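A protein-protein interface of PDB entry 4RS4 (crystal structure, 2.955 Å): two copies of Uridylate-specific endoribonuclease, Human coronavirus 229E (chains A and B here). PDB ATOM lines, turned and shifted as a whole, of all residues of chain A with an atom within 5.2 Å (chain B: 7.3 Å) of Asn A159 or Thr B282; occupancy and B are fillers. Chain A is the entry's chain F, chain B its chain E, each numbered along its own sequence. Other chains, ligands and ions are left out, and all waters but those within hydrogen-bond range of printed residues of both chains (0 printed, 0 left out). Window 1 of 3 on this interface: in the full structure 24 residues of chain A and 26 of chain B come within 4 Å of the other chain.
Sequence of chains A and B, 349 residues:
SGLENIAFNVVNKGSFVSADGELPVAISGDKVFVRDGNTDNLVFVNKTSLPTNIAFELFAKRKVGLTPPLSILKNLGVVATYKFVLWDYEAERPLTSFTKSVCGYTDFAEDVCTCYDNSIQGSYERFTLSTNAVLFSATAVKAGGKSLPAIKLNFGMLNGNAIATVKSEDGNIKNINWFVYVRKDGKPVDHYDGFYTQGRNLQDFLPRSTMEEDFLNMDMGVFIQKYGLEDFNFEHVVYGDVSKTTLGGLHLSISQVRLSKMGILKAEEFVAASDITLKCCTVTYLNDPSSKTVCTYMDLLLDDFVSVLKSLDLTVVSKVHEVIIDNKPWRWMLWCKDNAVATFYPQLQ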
ATOM      1  N   VAL A  64      22.250  -9.607  18.006  1.00  0.00           N
ATOM      2  CA  VAL A  64      22.303 -10.443  16.804  1.00  0.00           C
ATOM      3  C   VAL A  64      23.737 -10.539  16.296  1.00  0.00           C
ATOM      4  O   VAL A  64      24.564  -9.669  16.582  1.00  0.00           O
ATOM      5  CB  VAL A  64      21.393  -9.890  15.669  1.00  0.00           C
ATOM      6  CG1 VAL A  64      21.440 -10.792  14.453  1.00  0.00           C
ATOM      7  CG2 VAL A  64      19.962  -9.748  16.147  1.00  0.00           C
ATOM      8  N   GLY A  65      24.040 -11.611  15.568  1.00  0.00           N
ATOM      9  CA  GLY A  65      25.384 -11.814  15.068  1.00  0.00           C
ATOM     10  C   GLY A  65      26.279 -12.397  16.140  1.00  0.00           C
ATOM     11  O   GLY A  65      25.855 -13.254  16.915  1.00  0.00           O
ATOM     12  N   LEU A  66      27.528 -11.945  16.168  1.00  0.00           N
ATOM     13  CA  LEU A  66      28.483 -12.398  17.170  1.00  0.00           C
ATOM     14  C   LEU A  66      28.024 -12.040  18.588  1.00  0.00           C
ATOM     15  O   LEU A  66      27.742 -10.877  18.887  1.00  0.00           O
ATOM     16  CB  LEU A  66      29.864 -11.801  16.888  1.00  0.00           C
ATOM     17  CG  LEU A  66      30.511 -12.143  15.538  1.00  0.00           C
ATOM     18  CD1 LEU A  66      31.205 -10.926  14.926  1.00  0.00           C
ATOM     19  CD2 LEU A  66      31.483 -13.308  15.673  1.00  0.00           C
ATOM     20  N   THR A  67      27.953 -13.052  19.451  1.00  0.00           N
ATOM     21  CA  THR A  67      27.564 -12.875  20.849  1.00  0.00           C
ATOM     22  C   THR A  67      28.504 -13.653  21.754  1.00  0.00           C
ATOM     23  O   THR A  67      29.100 -14.643  21.326  1.00  0.00           O
ATOM     24  CB  THR A  67      26.116 -13.357  21.124  1.00  0.00           C
ATOM     25  OG1 THR A  67      25.959 -14.723  20.705  1.00  0.00           O
ATOM     26  CG2 THR A  67      25.109 -12.472  20.403  1.00  0.00           C
ATOM     27  N   TYR A  89      19.512 -19.713  22.373  1.00  0.00           N
ATOM     28  CA  TYR A  89      18.874 -20.340  21.221  1.00  0.00           C
ATOM     29  C   TYR A  89      18.598 -21.807  21.505  1.00  0.00           C
ATOM     30  O   TYR A  89      17.735 -22.423  20.883  1.00  0.00           O
ATOM     31  CB  TYR A  89      19.737 -20.198  19.974  1.00  0.00           C
ATOM     32  CG  TYR A  89      19.826 -18.793  19.418  1.00  0.00           C
ATOM     33  CD1 TYR A  89      19.073 -18.414  18.315  1.00  0.00           C
ATOM     34  CD2 TYR A  89      20.678 -17.852  19.981  1.00  0.00           C
ATOM     35  CE1 TYR A  89      19.159 -17.134  17.793  1.00  0.00           C
ATOM     36  CE2 TYR A  89      20.770 -16.572  19.465  1.00  0.00           C
ATOM     37  CZ  TYR A  89      20.007 -16.220  18.370  1.00  0.00           C
ATOM     38  OH  TYR A  89      20.091 -14.948  17.848  1.00  0.00           O
ATOM     39  N   MET A 157      29.758 -17.186  20.231  1.00  0.00           N
ATOM     40  CA  MET A 157      28.602 -17.668  19.485  1.00  0.00           C
ATOM     41  C   MET A 157      28.295 -16.767  18.298  1.00  0.00           C
ATOM     42  O   MET A 157      28.487 -15.552  18.360  1.00  0.00           O
ATOM     43  CB  MET A 157      27.379 -17.731  20.391  1.00  0.00           C
ATOM     44  CG  MET A 157      27.594 -18.541  21.647  1.00  0.00           C
ATOM     45  SD  MET A 157      27.856 -20.286  21.293  1.00  0.00           S
ATOM     46  CE  MET A 157      26.229 -20.745  20.716  1.00  0.00           C
ATOM     47  N   LEU A 158      27.823 -17.371  17.213  1.00  0.00           N
ATOM     48  CA  LEU A 158      27.390 -16.615  16.049  1.00  0.00           C
ATOM     49  C   LEU A 158      25.968 -17.023  15.682  1.00  0.00           C
ATOM     50  O   LEU A 158      25.730 -18.143  15.226  1.00  0.00           O
ATOM     51  CB  LEU A 158      28.340 -16.843  14.868  1.00  0.00           C
ATOM     52  CG  LEU A 158      28.024 -16.071  13.588  1.00  0.00           C
ATOM     53  CD1 LEU A 158      27.728 -14.614  13.910  1.00  0.00           C
ATOM     54  CD2 LEU A 158      29.181 -16.185  12.618  1.00  0.00           C
ATOM     55  N   ASN A 159      25.029 -16.101  15.871  1.00  0.00           N
ATOM     56  CA  ASN A 159      23.614 -16.370  15.626  1.00  0.00           C
ATOM     57  C   ASN A 159      23.116 -17.649  16.294  1.00  0.00           C
ATOM     58  O   ASN A 159      22.314 -18.389  15.721  1.00  0.00           O
ATOM     59  CB  ASN A 159      23.319 -16.395  14.122  1.00  0.00           C
ATOM     60  CG  ASN A 159      23.323 -15.010  13.507  1.00  0.00           C
ATOM     61  OD1 ASN A 159      22.624 -14.107  13.974  1.00  0.00           O
ATOM     62  ND2 ASN A 159      24.114 -14.833  12.457  1.00  0.00           N
ATOM     63  N   GLY A 160      23.592 -17.904  17.509  1.00  0.00           N
ATOM     64  CA  GLY A 160      23.192 -19.093  18.237  1.00  0.00           C
ATOM     65  C   GLY A 160      24.072 -20.310  18.003  1.00  0.00           C
ATOM     66  O   GLY A 160      23.897 -21.330  18.667  1.00  0.00           O
ATOM     67  N   ASN A 161      25.017 -20.214  17.072  1.00  0.00           N
ATOM     68  CA  ASN A 161      25.914 -21.333  16.770  1.00  0.00           C
ATOM     69  C   ASN A 161      27.331 -21.136  17.308  1.00  0.00           C
ATOM     70  O   ASN A 161      27.865 -20.030  17.272  1.00  0.00           O
ATOM     71  CB  ASN A 161      25.963 -21.582  15.262  1.00  0.00           C
ATOM     72  CG  ASN A 161      24.588 -21.693  14.650  1.00  0.00           C
ATOM     73  OD1 ASN A 161      23.978 -22.762  14.661  1.00  0.00           O
ATOM     74  ND2 ASN A 161      24.093 -20.588  14.106  1.00  0.00           N
ATOM     75  N   LEU B 247      29.481 -12.894   4.593  1.00  0.00           N
ATOM     76  CA  LEU B 247      29.522 -13.915   3.538  1.00  0.00           C
ATOM     77  C   LEU B 247      29.560 -13.396   2.098  1.00  0.00           C
ATOM     78  O   LEU B 247      30.563 -13.556   1.403  1.00  0.00           O
ATOM     79  CB  LEU B 247      28.348 -14.896   3.690  1.00  0.00           C
ATOM     80  CG  LEU B 247      28.625 -16.214   4.415  1.00  0.00           C
ATOM     81  CD1 LEU B 247      27.338 -16.970   4.698  1.00  0.00           C
ATOM     82  CD2 LEU B 247      29.585 -17.076   3.609  1.00  0.00           C
ATOM     83  N   LYS B 266      24.107 -23.126   8.445  1.00  0.00           N
ATOM     84  CA  LYS B 266      22.811 -22.989   9.090  1.00  0.00           C
ATOM     85  C   LYS B 266      22.037 -21.845   8.444  1.00  0.00           C
ATOM     86  O   LYS B 266      22.606 -20.799   8.133  1.00  0.00           O
ATOM     87  CB  LYS B 266      22.987 -22.755  10.595  1.00  0.00           C
ATOM     88  CG  LYS B 266      23.702 -23.893  11.327  1.00  0.00           C
ATOM     89  CD  LYS B 266      22.810 -25.122  11.473  1.00  0.00           C
ATOM     90  CE  LYS B 266      23.580 -26.318  12.024  1.00  0.00           C
ATOM     91  NZ  LYS B 266      22.666 -27.368  12.571  1.00  0.00           N
ATOM     92  N   ALA B 267      20.744 -22.058   8.226  1.00  0.00           N
ATOM     93  CA  ALA B 267      19.888 -21.028   7.650  1.00  0.00           C
ATOM     94  C   ALA B 267      18.581 -20.915   8.423  1.00  0.00           C
ATOM     95  O   ALA B 267      17.813 -21.876   8.497  1.00  0.00           O
ATOM     96  CB  ALA B 267      19.611 -21.320   6.178  1.00  0.00           C
ATOM     97  N   GLU B 268      18.335 -19.743   9.001  1.00  0.00           N
ATOM     98  CA  GLU B 268      17.065 -19.478   9.669  1.00  0.00           C
ATOM     99  C   GLU B 268      16.241 -18.481   8.868  1.00  0.00           C
ATOM    100  O   GLU B 268      16.576 -17.296   8.801  1.00  0.00           O
ATOM    101  CB  GLU B 268      17.287 -18.952  11.091  1.00  0.00           C
ATOM    102  CG  GLU B 268      17.600 -20.033  12.118  1.00  0.00           C
ATOM    103  CD  GLU B 268      16.444 -20.998  12.334  1.00  0.00           C
ATOM    104  OE1 GLU B 268      15.272 -20.568  12.240  1.00  0.00           O
ATOM    105  OE2 GLU B 268      16.710 -22.188  12.601  1.00  0.00           O
ATOM    106  N   GLU B 269      15.159 -18.961   8.267  1.00  0.00           N
ATOM    107  CA  GLU B 269      14.265 -18.080   7.529  1.00  0.00           C
ATOM    108  C   GLU B 269      13.472 -17.205   8.497  1.00  0.00           C
ATOM    109  O   GLU B 269      13.139 -17.635   9.604  1.00  0.00           O
ATOM    110  CB  GLU B 269      13.320 -18.886   6.632  1.00  0.00           C
ATOM    111  CG  GLU B 269      13.933 -19.328   5.303  1.00  0.00           C
ATOM    112  CD  GLU B 269      13.037 -19.014   4.113  1.00  0.00           C
ATOM    113  OE1 GLU B 269      12.479 -17.893   4.055  1.00  0.00           O
ATOM    114  OE2 GLU B 269      12.889 -19.890   3.236  1.00  0.00           O
ATOM    115  N   PHE B 270      13.187 -15.974   8.083  1.00  0.00           N
ATOM    116  CA  PHE B 270      12.380 -15.069   8.892  1.00  0.00           C
ATOM    117  C   PHE B 270      10.931 -15.533   8.876  1.00  0.00           C
ATOM    118  O   PHE B 270      10.277 -15.588   9.915  1.00  0.00           O
ATOM    119  CB  PHE B 270      12.499 -13.638   8.376  1.00  0.00           C
ATOM    120  CG  PHE B 270      13.907 -13.131   8.340  1.00  0.00           C
ATOM    121  CD1 PHE B 270      14.229 -11.989   7.621  1.00  0.00           C
ATOM    122  CD2 PHE B 270      14.916 -13.800   9.022  1.00  0.00           C
ATOM    123  CE1 PHE B 270      15.534 -11.520   7.587  1.00  0.00           C
ATOM    124  CE2 PHE B 270      16.220 -13.341   8.991  1.00  0.00           C
ATOM    125  CZ  PHE B 270      16.530 -12.197   8.273  1.00  0.00           C
ATOM    126  N   CYS B 280      14.079 -14.834   2.524  1.00  0.00           N
ATOM    127  CA  CYS B 280      15.041 -14.125   3.365  1.00  0.00           C
ATOM    128  C   CYS B 280      15.354 -14.909   4.638  1.00  0.00           C
ATOM    129  O   CYS B 280      14.436 -15.394   5.313  1.00  0.00           O
ATOM    130  CB  CYS B 280      14.505 -12.748   3.737  1.00  0.00           C
ATOM    131  SG  CYS B 280      15.779 -11.484   3.786  1.00  0.00           S
ATOM    132  N   CYS B 281      16.641 -15.034   4.961  1.00  0.00           N
ATOM    133  CA  CYS B 281      17.077 -15.812   6.114  1.00  0.00           C
ATOM    134  C   CYS B 281      18.410 -15.282   6.633  1.00  0.00           C
ATOM    135  O   CYS B 281      19.138 -14.602   5.913  1.00  0.00           O
ATOM    136  CB  CYS B 281      17.275 -17.268   5.703  1.00  0.00           C
ATOM    137  SG  CYS B 281      18.795 -17.517   4.758  1.00  0.00           S
ATOM    138  N   THR B 282      18.746 -15.621   7.872  1.00  0.00           N
ATOM    139  CA  THR B 282      20.090 -15.379   8.387  1.00  0.00           C
ATOM    140  C   THR B 282      20.941 -16.622   8.122  1.00  0.00           C
ATOM    141  O   THR B 282      20.554 -17.738   8.476  1.00  0.00           O
ATOM    142  CB  THR B 282      20.064 -15.089   9.895  1.00  0.00           C
ATOM    143  OG1 THR B 282      19.080 -14.086  10.168  1.00  0.00           O
ATOM    144  CG2 THR B 282      21.420 -14.608  10.367  1.00  0.00           C
ATOM    145  N   VAL B 283      22.093 -16.437   7.488  1.00  0.00           N
ATOM    146  CA  VAL B 283      22.945 -17.574   7.159  1.00  0.00           C
ATOM    147  C   VAL B 283      24.207 -17.563   8.010  1.00  0.00           C
ATOM    148  O   VAL B 283      24.785 -16.506   8.264  1.00  0.00           O
ATOM    149  CB  VAL B 283      23.336 -17.587   5.670  1.00  0.00           C
ATOM    150  CG1 VAL B 283      23.920 -18.934   5.299  1.00  0.00           C
ATOM    151  CG2 VAL B 283      22.128 -17.289   4.803  1.00  0.00           C
ATOM    152  N   THR B 284      24.630 -18.744   8.448  1.00  0.00           N
ATOM    153  CA  THR B 284      25.854 -18.864   9.235  1.00  0.00           C
ATOM    154  C   THR B 284      26.699 -20.070   8.797  1.00  0.00           C
ATOM    155  O   THR B 284      26.168 -21.141   8.483  1.00  0.00           O
ATOM    156  CB  THR B 284      25.544 -18.953  10.741  1.00  0.00           C
ATOM    157  OG1 THR B 284      24.581 -17.950  11.100  1.00  0.00           O
ATOM    158  CG2 THR B 284      26.809 -18.744  11.547  1.00  0.00           C
ATOM    159  N   SER B 290      31.441 -17.264   9.292  1.00  0.00           N
ATOM    160  CA  SER B 290      30.961 -16.169   8.468  1.00  0.00           C
ATOM    161  C   SER B 290      29.440 -16.146   8.524  1.00  0.00           C
ATOM    162  O   SER B 290      28.801 -17.179   8.747  1.00  0.00           O
ATOM    163  CB  SER B 290      31.424 -16.353   7.026  1.00  0.00           C
ATOM    164  OG  SER B 290      31.098 -15.224   6.228  1.00  0.00           O
ATOM    165  N   SER B 291      28.860 -14.972   8.308  1.00  0.00           N
ATOM    166  CA  SER B 291      27.418 -14.809   8.430  1.00  0.00           C
ATOM    167  C   SER B 291      26.899 -13.751   7.472  1.00  0.00           C
ATOM    168  O   SER B 291      27.643 -12.875   7.041  1.00  0.00           O
ATOM    169  CB  SER B 291      27.058 -14.416   9.867  1.00  0.00           C
ATOM    170  OG  SER B 291      27.981 -13.468  10.387  1.00  0.00           O
ATOM    171  N   LYS B 292      25.626 -13.858   7.114  1.00  0.00           N
ATOM    172  CA  LYS B 292      24.923 -12.770   6.456  1.00  0.00           C
ATOM    173  C   LYS B 292      23.605 -12.597   7.201  1.00  0.00           C
ATOM    174  O   LYS B 292      22.730 -13.465   7.136  1.00  0.00           O
ATOM    175  CB  LYS B 292      24.686 -13.096   4.977  1.00  0.00           C
ATOM    176  CG  LYS B 292      24.017 -11.978   4.188  1.00  0.00           C
ATOM    177  CD  LYS B 292      24.787 -11.672   2.914  1.00  0.00           C
ATOM    178  CE  LYS B 292      24.153 -10.519   2.141  1.00  0.00           C
ATOM    179  NZ  LYS B 292      24.861 -10.203   0.862  1.00  0.00           N
ATOM    180  N   THR B 293      23.454 -11.473   7.896  1.00  0.00           N
ATOM    181  CA  THR B 293      22.277 -11.263   8.736  1.00  0.00           C
ATOM    182  C   THR B 293      20.991 -11.229   7.908  1.00  0.00           C
ATOM    183  O   THR B 293      20.010 -11.904   8.233  1.00  0.00           O
ATOM    184  CB  THR B 293      22.398  -9.988   9.599  1.00  0.00           C
ATOM    185  OG1 THR B 293      23.519 -10.115  10.483  1.00  0.00           O
ATOM    186  CG2 THR B 293      21.137  -9.777  10.428  1.00  0.00           C
ATOM    187  N   VAL B 294      20.995 -10.434   6.842  1.00  0.00           N
ATOM    188  CA  VAL B 294      19.883 -10.445   5.901  1.00  0.00           C
ATOM    189  C   VAL B 294      20.335 -10.968   4.551  1.00  0.00           C
ATOM    190  O   VAL B 294      21.061 -10.304   3.815  1.00  0.00           O
ATOM    191  CB  VAL B 294      19.243  -9.056   5.743  1.00  0.00           C
ATOM    192  CG1 VAL B 294      18.191  -9.085   4.651  1.00  0.00           C
ATOM    193  CG2 VAL B 294      18.630  -8.611   7.058  1.00  0.00           C
ATOM    194  N   CYS B 295      19.899 -12.178   4.239  1.00  0.00           N
ATOM    195  CA  CYS B 295      20.318 -12.855   3.028  1.00  0.00           C
ATOM    196  C   CYS B 295      19.087 -13.168   2.207  1.00  0.00           C
ATOM    197  O   CYS B 295      18.275 -14.011   2.596  1.00  0.00           O
ATOM    198  CB  CYS B 295      21.062 -14.138   3.403  1.00  0.00           C
ATOM    199  SG  CYS B 295      21.470 -15.249   2.040  1.00  0.00           S
ATOM    200  N   TYR B 297      17.315 -14.700  -1.103  1.00  0.00           N
ATOM    201  CA  TYR B 297      17.623 -15.747  -2.073  1.00  0.00           C
ATOM    202  C   TYR B 297      16.385 -16.308  -2.784  1.00  0.00           C
ATOM    203  O   TYR B 297      15.253 -16.094  -2.350  1.00  0.00           O
ATOM    204  CB  TYR B 297      18.452 -16.858  -1.431  1.00  0.00           C
ATOM    205  CG  TYR B 297      17.728 -17.626  -0.361  1.00  0.00           C
ATOM    206  CD1 TYR B 297      17.190 -18.881  -0.623  1.00  0.00           C
ATOM    207  CD2 TYR B 297      17.576 -17.099   0.910  1.00  0.00           C
ATOM    208  CE1 TYR B 297      16.525 -19.592   0.358  1.00  0.00           C
ATOM    209  CE2 TYR B 297      16.914 -17.802   1.896  1.00  0.00           C
ATOM    210  CZ  TYR B 297      16.391 -19.049   1.616  1.00  0.00           C
ATOM    211  OH  TYR B 297      15.731 -19.757   2.597  1.00  0.00           O
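The side-chain hydroxyl of Thr B284 lies within hydrogen-bond range of the side-chain amide nitrogen of Asn A159, 3.4 Å away.
Among the printed residues, merely in contact across the chains: Asn A159 with Thr B282 (3.4 Å), Asn A161 with Lys B266 (3.5 Å), Leu A158 with Thr B284 (3.6 Å), Leu A158 with Ser B291 (3.7 Å) and Asn A159 with Ser B291 (3.9 Å).
The backbone carbonyl oxygen (O) of Leu A158 lies within hydrogen-bond range of the side-chain amide nitrogen (ND2) of Asn A161.
The side-chain hydroxyl (OG1) of Thr B282 sits at hydrogen-bond distance from the backbone carbonyl oxygen (O) of Thr B293 (3.1 Å).
O of Gly A65 sits at hydrogen-bond distance from N of Asn A159 (3.1 Å).
The backbone carbonyl oxygen of Thr B284 lies within hydrogen-bond range of the backbone NH of Lys B266.
The backbone NH (N) of Thr B282 lies within hydrogen-bond range of the backbone carbonyl oxygen (O) of Glu B268.
O of Asn A159 lies within hydrogen-bond range of ND2 of Asn A161, 3.3 Å away.
No position is printed for both chains.
Asn A159 touches just these residues of chain B: Thr B282 (3.4 Å), Thr B284 (3.4 Å) and Ser B291 (3.9 Å).
Printed residues of chain A within 4 Å of Thr B282: Asn A159 (3.4 Å).
Of the printed residues of chain A, Ser B291 touches Leu A158 (3.7 Å) and Asn A159 (3.9 Å).
Of the printed residues of chain A, Thr B284 touches Leu A158 and Asn A159.
Of the printed residues of chain B, Leu A158 touches Thr B284 and Ser B291.
Of the printed residues of chain A, Lys B266 touches Asn A161 (3.5 Å).
Val A64 touches none of the printed residues of chain B.
Tyr A89 touches none of the printed residues of chain B.
The nearest printed residue of chain A that does not touch Thr B282 is Val A64 (5.6 Å).
Of the 10 printed residues of chain A, 3 touch a printed residue of chain B.
Hydrophobic or aromatic side chains of chain A within 4 Å of the printed part of chain B: Leu A158.
Among the printed residues, 6 pairs touch across the chains.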
